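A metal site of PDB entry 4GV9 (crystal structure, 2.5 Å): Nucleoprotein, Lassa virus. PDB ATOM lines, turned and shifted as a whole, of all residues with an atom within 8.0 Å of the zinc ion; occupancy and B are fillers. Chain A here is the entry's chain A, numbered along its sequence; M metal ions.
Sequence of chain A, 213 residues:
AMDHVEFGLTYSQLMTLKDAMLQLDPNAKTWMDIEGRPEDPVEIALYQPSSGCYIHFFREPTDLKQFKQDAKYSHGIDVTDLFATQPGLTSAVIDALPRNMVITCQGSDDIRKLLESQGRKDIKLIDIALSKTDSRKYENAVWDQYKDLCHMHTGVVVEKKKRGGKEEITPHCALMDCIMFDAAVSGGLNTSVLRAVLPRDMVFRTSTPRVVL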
ATOM      1  N   GLU A  35     -16.977  -6.368  33.297  1.00  0.00           N
ATOM      2  CA  GLU A  35     -15.557  -6.101  33.472  1.00  0.00           C
ATOM      3  C   GLU A  35     -15.336  -5.541  34.873  1.00  0.00           C
ATOM      4  O   GLU A  35     -16.176  -4.808  35.393  1.00  0.00           O
ATOM      5  CB  GLU A  35     -15.017  -5.155  32.392  1.00  0.00           C
ATOM      6  CG  GLU A  35     -15.144  -5.684  30.965  1.00  0.00           C
ATOM      7  CD  GLU A  35     -14.557  -7.072  30.767  1.00  0.00           C
ATOM      8  OE1 GLU A  35     -13.434  -7.340  31.255  1.00  0.00           O
ATOM      9  OE2 GLU A  35     -15.224  -7.896  30.115  1.00  0.00           O
ATOM     10  N   GLU A  43     -17.716  -2.204  34.318  1.00  0.00           N
ATOM     11  CA  GLU A  43     -18.482  -2.232  33.072  1.00  0.00           C
ATOM     12  C   GLU A  43     -19.455  -3.398  33.086  1.00  0.00           C
ATOM     13  O   GLU A  43     -19.079  -4.527  33.374  1.00  0.00           O
ATOM     14  CB  GLU A  43     -17.557  -2.324  31.858  1.00  0.00           C
ATOM     15  CG  GLU A  43     -18.270  -2.184  30.520  1.00  0.00           C
ATOM     16  CD  GLU A  43     -17.361  -2.374  29.319  1.00  0.00           C
ATOM     17  OE1 GLU A  43     -16.436  -3.217  29.387  1.00  0.00           O
ATOM     18  OE2 GLU A  43     -17.567  -1.686  28.302  1.00  0.00           O
ATOM     19  N   ILE A  44     -20.727  -3.104  32.792  1.00  0.00           N
ATOM     20  CA  ILE A  44     -21.776  -4.119  32.768  1.00  0.00           C
ATOM     21  C   ILE A  44     -22.540  -4.071  31.450  1.00  0.00           C
ATOM     22  O   ILE A  44     -22.932  -2.989  30.983  1.00  0.00           O
ATOM     23  CB  ILE A  44     -22.750  -3.963  33.966  1.00  0.00           C
ATOM     24  CG1 ILE A  44     -22.005  -4.195  35.282  1.00  0.00           C
ATOM     25  CG2 ILE A  44     -23.926  -4.916  33.845  1.00  0.00           C
ATOM     26  CD1 ILE A  44     -22.653  -3.560  36.482  1.00  0.00           C
ATOM     27  N   ALA A  45     -22.736  -5.232  30.834  1.00  0.00           N
ATOM     28  CA  ALA A  45     -23.481  -5.333  29.593  1.00  0.00           C
ATOM     29  C   ALA A  45     -24.418  -6.520  29.559  1.00  0.00           C
ATOM     30  O   ALA A  45     -24.081  -7.615  30.025  1.00  0.00           O
ATOM     31  CB  ALA A  45     -22.536  -5.363  28.404  1.00  0.00           C
ATOM     32  N   HIS A  56     -25.787  -1.311  28.346  1.00  0.00           N
ATOM     33  CA  HIS A  56     -24.351  -1.068  28.497  1.00  0.00           C
ATOM     34  C   HIS A  56     -24.076   0.190  29.305  1.00  0.00           C
ATOM     35  O   HIS A  56     -24.442   1.292  28.903  1.00  0.00           O
ATOM     36  CB  HIS A  56     -23.665  -1.008  27.127  1.00  0.00           C
ATOM     37  CG  HIS A  56     -22.180  -0.817  27.195  1.00  0.00           C
ATOM     38  ND1 HIS A  56     -21.516   0.088  26.395  1.00  0.00           N
ATOM     39  CD2 HIS A  56     -21.235  -1.401  27.974  1.00  0.00           C
ATOM     40  CE1 HIS A  56     -20.224   0.047  26.674  1.00  0.00           C
ATOM     41  NE2 HIS A  56     -20.034  -0.847  27.626  1.00  0.00           N
ATOM     42  N   PHE A  57     -23.431   0.015  30.460  1.00  0.00           N
ATOM     43  CA  PHE A  57     -23.105   1.127  31.360  1.00  0.00           C
ATOM     44  C   PHE A  57     -21.863   0.857  32.200  1.00  0.00           C
ATOM     45  O   PHE A  57     -21.349  -0.263  32.241  1.00  0.00           O
ATOM     46  CB  PHE A  57     -24.306   1.486  32.249  1.00  0.00           C
ATOM     47  CG  PHE A  57     -24.751   0.371  33.168  1.00  0.00           C
ATOM     48  CD1 PHE A  57     -25.641  -0.601  32.727  1.00  0.00           C
ATOM     49  CD2 PHE A  57     -24.288   0.311  34.473  1.00  0.00           C
ATOM     50  CE1 PHE A  57     -26.051  -1.616  33.575  1.00  0.00           C
ATOM     51  CE2 PHE A  57     -24.697  -0.703  35.320  1.00  0.00           C
ATOM     52  CZ  PHE A  57     -25.576  -1.670  34.873  1.00  0.00           C
ATOM     53  N   PHE A  58     -21.382   1.905  32.867  1.00  0.00           N
ATOM     54  CA  PHE A  58     -20.117   1.857  33.608  1.00  0.00           C
ATOM     55  C   PHE A  58     -20.284   2.268  35.068  1.00  0.00           C
ATOM     56  O   PHE A  58     -21.280   2.902  35.428  1.00  0.00           O
ATOM     57  CB  PHE A  58     -19.071   2.746  32.927  1.00  0.00           C
ATOM     58  CG  PHE A  58     -18.854   2.435  31.468  1.00  0.00           C
ATOM     59  CD1 PHE A  58     -19.625   3.061  30.489  1.00  0.00           C
ATOM     60  CD2 PHE A  58     -17.868   1.539  31.085  1.00  0.00           C
ATOM     61  CE1 PHE A  58     -19.430   2.771  29.150  1.00  0.00           C
ATOM     62  CE2 PHE A  58     -17.670   1.249  29.737  1.00  0.00           C
ATOM     63  CZ  PHE A  58     -18.448   1.875  28.776  1.00  0.00           C
ATOM     64  N   HIS A  75      -9.390  -5.506  30.801  1.00  0.00           N
ATOM     65  CA  HIS A  75     -10.253  -4.507  30.163  1.00  0.00           C
ATOM     66  C   HIS A  75      -9.571  -3.283  29.539  1.00  0.00           C
ATOM     67  O   HIS A  75     -10.009  -2.795  28.502  1.00  0.00           O
ATOM     68  CB  HIS A  75     -11.430  -4.087  31.067  1.00  0.00           C
ATOM     69  CG  HIS A  75     -11.034  -3.728  32.467  1.00  0.00           C
ATOM     70  ND1 HIS A  75     -10.249  -2.640  32.772  1.00  0.00           N
ATOM     71  CD2 HIS A  75     -11.349  -4.299  33.656  1.00  0.00           C
ATOM     72  CE1 HIS A  75     -10.086  -2.561  34.083  1.00  0.00           C
ATOM     73  NE2 HIS A  75     -10.744  -3.562  34.641  1.00  0.00           N
ATOM     74  N   ILE A  77      -9.412  -0.222  30.673  1.00  0.00           N
ATOM     75  CA  ILE A  77     -10.210   0.986  30.859  1.00  0.00           C
ATOM     76  C   ILE A  77      -9.391   2.049  31.578  1.00  0.00           C
ATOM     77  O   ILE A  77      -8.766   1.780  32.602  1.00  0.00           O
ATOM     78  CB  ILE A  77     -11.511   0.696  31.643  1.00  0.00           C
ATOM     79  CG1 ILE A  77     -12.353  -0.378  30.936  1.00  0.00           C
ATOM     80  CG2 ILE A  77     -12.334   1.979  31.832  1.00  0.00           C
ATOM     81  CD1 ILE A  77     -13.471  -0.967  31.776  1.00  0.00           C
ATOM     82  N   TRP A 143     -15.482  -6.709  16.782  1.00  0.00           N
ATOM     83  CA  TRP A 143     -14.846  -5.396  16.889  1.00  0.00           C
ATOM     84  C   TRP A 143     -14.859  -4.638  15.556  1.00  0.00           C
ATOM     85  O   TRP A 143     -14.944  -3.408  15.543  1.00  0.00           O
ATOM     86  CB  TRP A 143     -13.407  -5.517  17.406  1.00  0.00           C
ATOM     87  CG  TRP A 143     -13.302  -5.718  18.893  1.00  0.00           C
ATOM     88  CD1 TRP A 143     -13.221  -6.916  19.551  1.00  0.00           C
ATOM     89  CD2 TRP A 143     -13.277  -4.698  19.898  1.00  0.00           C
ATOM     90  NE1 TRP A 143     -13.138  -6.697  20.899  1.00  0.00           N
ATOM     91  CE2 TRP A 143     -13.166  -5.358  21.145  1.00  0.00           C
ATOM     92  CE3 TRP A 143     -13.319  -3.303  19.866  1.00  0.00           C
ATOM     93  CZ2 TRP A 143     -13.109  -4.656  22.359  1.00  0.00           C
ATOM     94  CZ3 TRP A 143     -13.258  -2.602  21.072  1.00  0.00           C
ATOM     95  CH2 TRP A 143     -13.165  -3.281  22.301  1.00  0.00           C
ATOM     96  N   LYS A 147     -17.216  -1.595  16.933  1.00  0.00           N
ATOM     97  CA  LYS A 147     -16.218  -0.790  17.659  1.00  0.00           C
ATOM     98  C   LYS A 147     -16.706   0.582  18.145  1.00  0.00           C
ATOM     99  O   LYS A 147     -16.249   1.076  19.174  1.00  0.00           O
ATOM    100  CB  LYS A 147     -14.934  -0.621  16.834  1.00  0.00           C
ATOM    101  CG  LYS A 147     -15.109   0.086  15.499  1.00  0.00           C
ATOM    102  CD  LYS A 147     -13.763   0.403  14.865  1.00  0.00           C
ATOM    103  CE  LYS A 147     -13.933   1.160  13.549  1.00  0.00           C
ATOM    104  NZ  LYS A 147     -14.508   0.301  12.468  1.00  0.00           N
ATOM    105  N   LEU A 149     -19.448   1.374  19.443  1.00  0.00           N
ATOM    106  CA  LEU A 149     -20.339   1.275  20.603  1.00  0.00           C
ATOM    107  C   LEU A 149     -19.620   1.426  21.948  1.00  0.00           C
ATOM    108  O   LEU A 149     -20.268   1.640  22.978  1.00  0.00           O
ATOM    109  CB  LEU A 149     -21.145  -0.029  20.562  1.00  0.00           C
ATOM    110  CG  LEU A 149     -22.045  -0.295  19.344  1.00  0.00           C
ATOM    111  CD1 LEU A 149     -22.628  -1.701  19.424  1.00  0.00           C
ATOM    112  CD2 LEU A 149     -23.154   0.733  19.197  1.00  0.00           C
ATOM    113  N   CYS A 150     -18.292   1.306  21.941  1.00  0.00           N
ATOM    114  CA  CYS A 150     -17.495   1.471  23.155  1.00  0.00           C
ATOM    115  C   CYS A 150     -16.091   2.022  22.855  1.00  0.00           C
ATOM    116  O   CYS A 150     -15.348   1.440  22.056  1.00  0.00           O
ATOM    117  CB  CYS A 150     -17.383   0.144  23.916  1.00  0.00           C
ATOM    118  SG  CYS A 150     -16.751   0.312  25.605  1.00  0.00           S
ATOM    119  N   HIS A 151     -15.754   3.137  23.495  1.00  0.00           N
ATOM    120  CA  HIS A 151     -14.458   3.805  23.289  1.00  0.00           C
ATOM    121  C   HIS A 151     -13.564   3.737  24.525  1.00  0.00           C
ATOM    122  O   HIS A 151     -12.451   4.287  24.534  1.00  0.00           O
ATOM    123  CB  HIS A 151     -14.661   5.272  22.893  1.00  0.00           C
ATOM    124  CG  HIS A 151     -15.535   5.474  21.698  1.00  0.00           C
ATOM    125  ND1 HIS A 151     -15.504   4.658  20.589  1.00  0.00           N
ATOM    126  CD2 HIS A 151     -16.464   6.425  21.430  1.00  0.00           C
ATOM    127  CE1 HIS A 151     -16.385   5.087  19.699  1.00  0.00           C
ATOM    128  NE2 HIS A 151     -16.977   6.165  20.188  1.00  0.00           N
ATOM    129  N   MET A 152     -14.034   3.059  25.567  1.00  0.00           N
ATOM    130  CA  MET A 152     -13.415   3.108  26.899  1.00  0.00           C
ATOM    131  C   MET A 152     -12.100   2.339  27.036  1.00  0.00           C
ATOM    132  O   MET A 152     -11.315   2.615  27.947  1.00  0.00           O
ATOM    133  CB  MET A 152     -14.418   2.627  27.956  1.00  0.00           C
ATOM    134  CG  MET A 152     -15.549   3.609  28.201  1.00  0.00           C
ATOM    135  SD  MET A 152     -15.093   4.934  29.326  1.00  0.00           S
ATOM    136  CE  MET A 152     -16.209   6.227  28.799  1.00  0.00           C
ATOM    137  N   HIS A 153     -11.863   1.404  26.131  1.00  0.00           N
ATOM    138  CA  HIS A 153     -10.696   0.524  26.224  1.00  0.00           C
ATOM    139  C   HIS A 153      -9.523   1.056  25.403  1.00  0.00           C
ATOM    140  O   HIS A 153      -9.333   0.696  24.245  1.00  0.00           O
ATOM    141  CB  HIS A 153     -11.083  -0.904  25.822  1.00  0.00           C
ATOM    142  CG  HIS A 153     -12.348  -1.382  26.464  1.00  0.00           C
ATOM    143  ND1 HIS A 153     -12.403  -1.839  27.760  1.00  0.00           N
ATOM    144  CD2 HIS A 153     -13.616  -1.458  25.988  1.00  0.00           C
ATOM    145  CE1 HIS A 153     -13.649  -2.175  28.056  1.00  0.00           C
ATOM    146  NE2 HIS A 153     -14.394  -1.956  26.994  1.00  0.00           N
ATOM    147  N   PRO A 171      -8.307  -5.664  24.026  1.00  0.00           N
ATOM    148  CA  PRO A 171      -8.926  -5.443  25.334  1.00  0.00           C
ATOM    149  C   PRO A 171     -10.298  -6.082  25.491  1.00  0.00           C
ATOM    150  O   PRO A 171     -11.035  -6.224  24.512  1.00  0.00           O
ATOM    151  CB  PRO A 171      -9.037  -3.920  25.414  1.00  0.00           C
ATOM    152  CG  PRO A 171      -7.956  -3.414  24.532  1.00  0.00           C
ATOM    153  CD  PRO A 171      -7.899  -4.392  23.395  1.00  0.00           C
ATOM    154  N   HIS A 172     -10.629  -6.449  26.731  1.00  0.00           N
ATOM    155  CA  HIS A 172     -11.900  -7.102  27.057  1.00  0.00           C
ATOM    156  C   HIS A 172     -13.007  -6.075  27.275  1.00  0.00           C
ATOM    157  O   HIS A 172     -12.896  -5.214  28.157  1.00  0.00           O
ATOM    158  CB  HIS A 172     -11.739  -7.967  28.314  1.00  0.00           C
ATOM    159  CG  HIS A 172     -11.000  -9.247  28.086  1.00  0.00           C
ATOM    160  ND1 HIS A 172     -11.200 -10.362  28.862  1.00  0.00           N
ATOM    161  CD2 HIS A 172     -10.072  -9.593  27.161  1.00  0.00           C
ATOM    162  CE1 HIS A 172     -10.416 -11.342  28.439  1.00  0.00           C
ATOM    163  NE2 HIS A 172      -9.724 -10.906  27.399  1.00  0.00           N
ATOM    164  N   CYS A 173     -14.059  -6.170  26.479  1.00  0.00           N
ATOM    165  CA  CYS A 173     -15.230  -5.329  26.641  1.00  0.00           C
ATOM    166  C   CYS A 173     -16.443  -6.181  26.979  1.00  0.00           C
ATOM    167  O   CYS A 173     -16.704  -7.186  26.319  1.00  0.00           O
ATOM    168  CB  CYS A 173     -15.497  -4.537  25.356  1.00  0.00           C
ATOM    169  SG  CYS A 173     -16.915  -3.418  25.457  1.00  0.00           S
ATOM    170  N   ALA A 174     -17.180  -5.785  28.008  1.00  0.00           N
ATOM    171  CA  ALA A 174     -18.366  -6.508  28.456  1.00  0.00           C
ATOM    172  C   ALA A 174     -19.413  -6.651  27.348  1.00  0.00           C
ATOM    173  O   ALA A 174     -20.060  -7.699  27.244  1.00  0.00           O
ATOM    174  CB  ALA A 174     -18.973  -5.820  29.680  1.00  0.00           C
ATOM    175  N   LEU A 175     -19.557  -5.614  26.534  1.00  0.00           N
ATOM    176  CA  LEU A 175     -20.514  -5.619  25.420  1.00  0.00           C
ATOM    177  C   LEU A 175     -20.034  -6.488  24.255  1.00  0.00           C
ATOM    178  O   LEU A 175     -20.804  -7.294  23.731  1.00  0.00           O
ATOM    179  CB  LEU A 175     -20.824  -4.192  24.957  1.00  0.00           C
ATOM    180  CG  LEU A 175     -21.823  -3.979  23.815  1.00  0.00           C
ATOM    181  CD1 LEU A 175     -23.185  -4.585  24.128  1.00  0.00           C
ATOM    182  CD2 LEU A 175     -21.963  -2.503  23.489  1.00  0.00           C
ATOM    183  N   MET A 176     -18.774  -6.321  23.872  1.00  0.00           N
ATOM    184  CA  MET A 176     -18.190  -7.080  22.765  1.00  0.00           C
ATOM    185  C   MET A 176     -18.092  -8.571  23.094  1.00  0.00           C
ATOM    186  O   MET A 176     -18.272  -9.415  22.213  1.00  0.00           O
ATOM    187  CB  MET A 176     -16.802  -6.537  22.381  1.00  0.00           C
ATOM    188  CG  MET A 176     -16.766  -5.056  22.047  1.00  0.00           C
ATOM    189  SD  MET A 176     -17.899  -4.554  20.739  1.00  0.00           S
ATOM    190  CE  MET A 176     -18.123  -2.832  21.179  1.00  0.00           C
ATOM    191  N   ASP A 177     -17.828  -8.878  24.365  1.00  0.00           N
ATOM    192  CA  ASP A 177     -17.812 -10.260  24.846  1.00  0.00           C
ATOM    193  C   ASP A 177     -19.165 -10.929  24.651  1.00  0.00           C
ATOM    194  O   ASP A 177     -19.244 -12.037  24.116  1.00  0.00           O
ATOM    195  CB  ASP A 177     -17.373 -10.325  26.305  1.00  0.00           C
ATOM    196  CG  ASP A 177     -15.861 -10.212  26.481  1.00  0.00           C
ATOM    197  OD1 ASP A 177     -15.145  -9.964  25.481  1.00  0.00           O
ATOM    198  OD2 ASP A 177     -15.383 -10.380  27.627  1.00  0.00           O
HETATM  199 ZN    ZN M   1     -16.562  -1.654  26.506  1.00  0.00          ZN
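A ring nitrogen (NE2) of His 56 sits close to the side-chain carboxylate (OE2) of Glu 43 (2.7 Å).
The backbone NH of Ala 174 is in hydrogen-bond range of the side-chain carboxylate of Glu 43, at 3.0 Å.
O of Glu 43 lies within hydrogen-bond range of N of Glu 35, at 2.8 Å.
N of Leu 175 lies close to SG of Cys 173, 3.6 Å away.
The side-chain sulfur (SG) of Cys 173 sits close to the backbone NH (N) of Met 176 (3.8 Å).
A ring nitrogen (ND1) of His 153 lies close to the backbone carbonyl oxygen (O) of His 172 (3.4 Å).
The backbone carbonyl oxygen of His 75 sits at hydrogen-bond distance from a ring nitrogen (ND1) of His 153 (2.7 Å).
Residues that only touch the zinc ion: His 56.
Of the 23 residues printed, 5 come within 4 Å of the zinc ion.
The nearest printed residue that does not touch the zinc ion is Ala 174 (4.4 Å).
The zinc ion is bound by the side-chain carboxylate (OE2) of Glu 43 (2.1 Å), the side-chain sulfur (SG) of Cys 173 (2.1 Å), the side-chain sulfur (SG) of Cys 150 (2.2 Å) and a ring nitrogen (NE2) of His 153 (2.2 Å).
The zinc ion has four donor atoms within binding distance.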
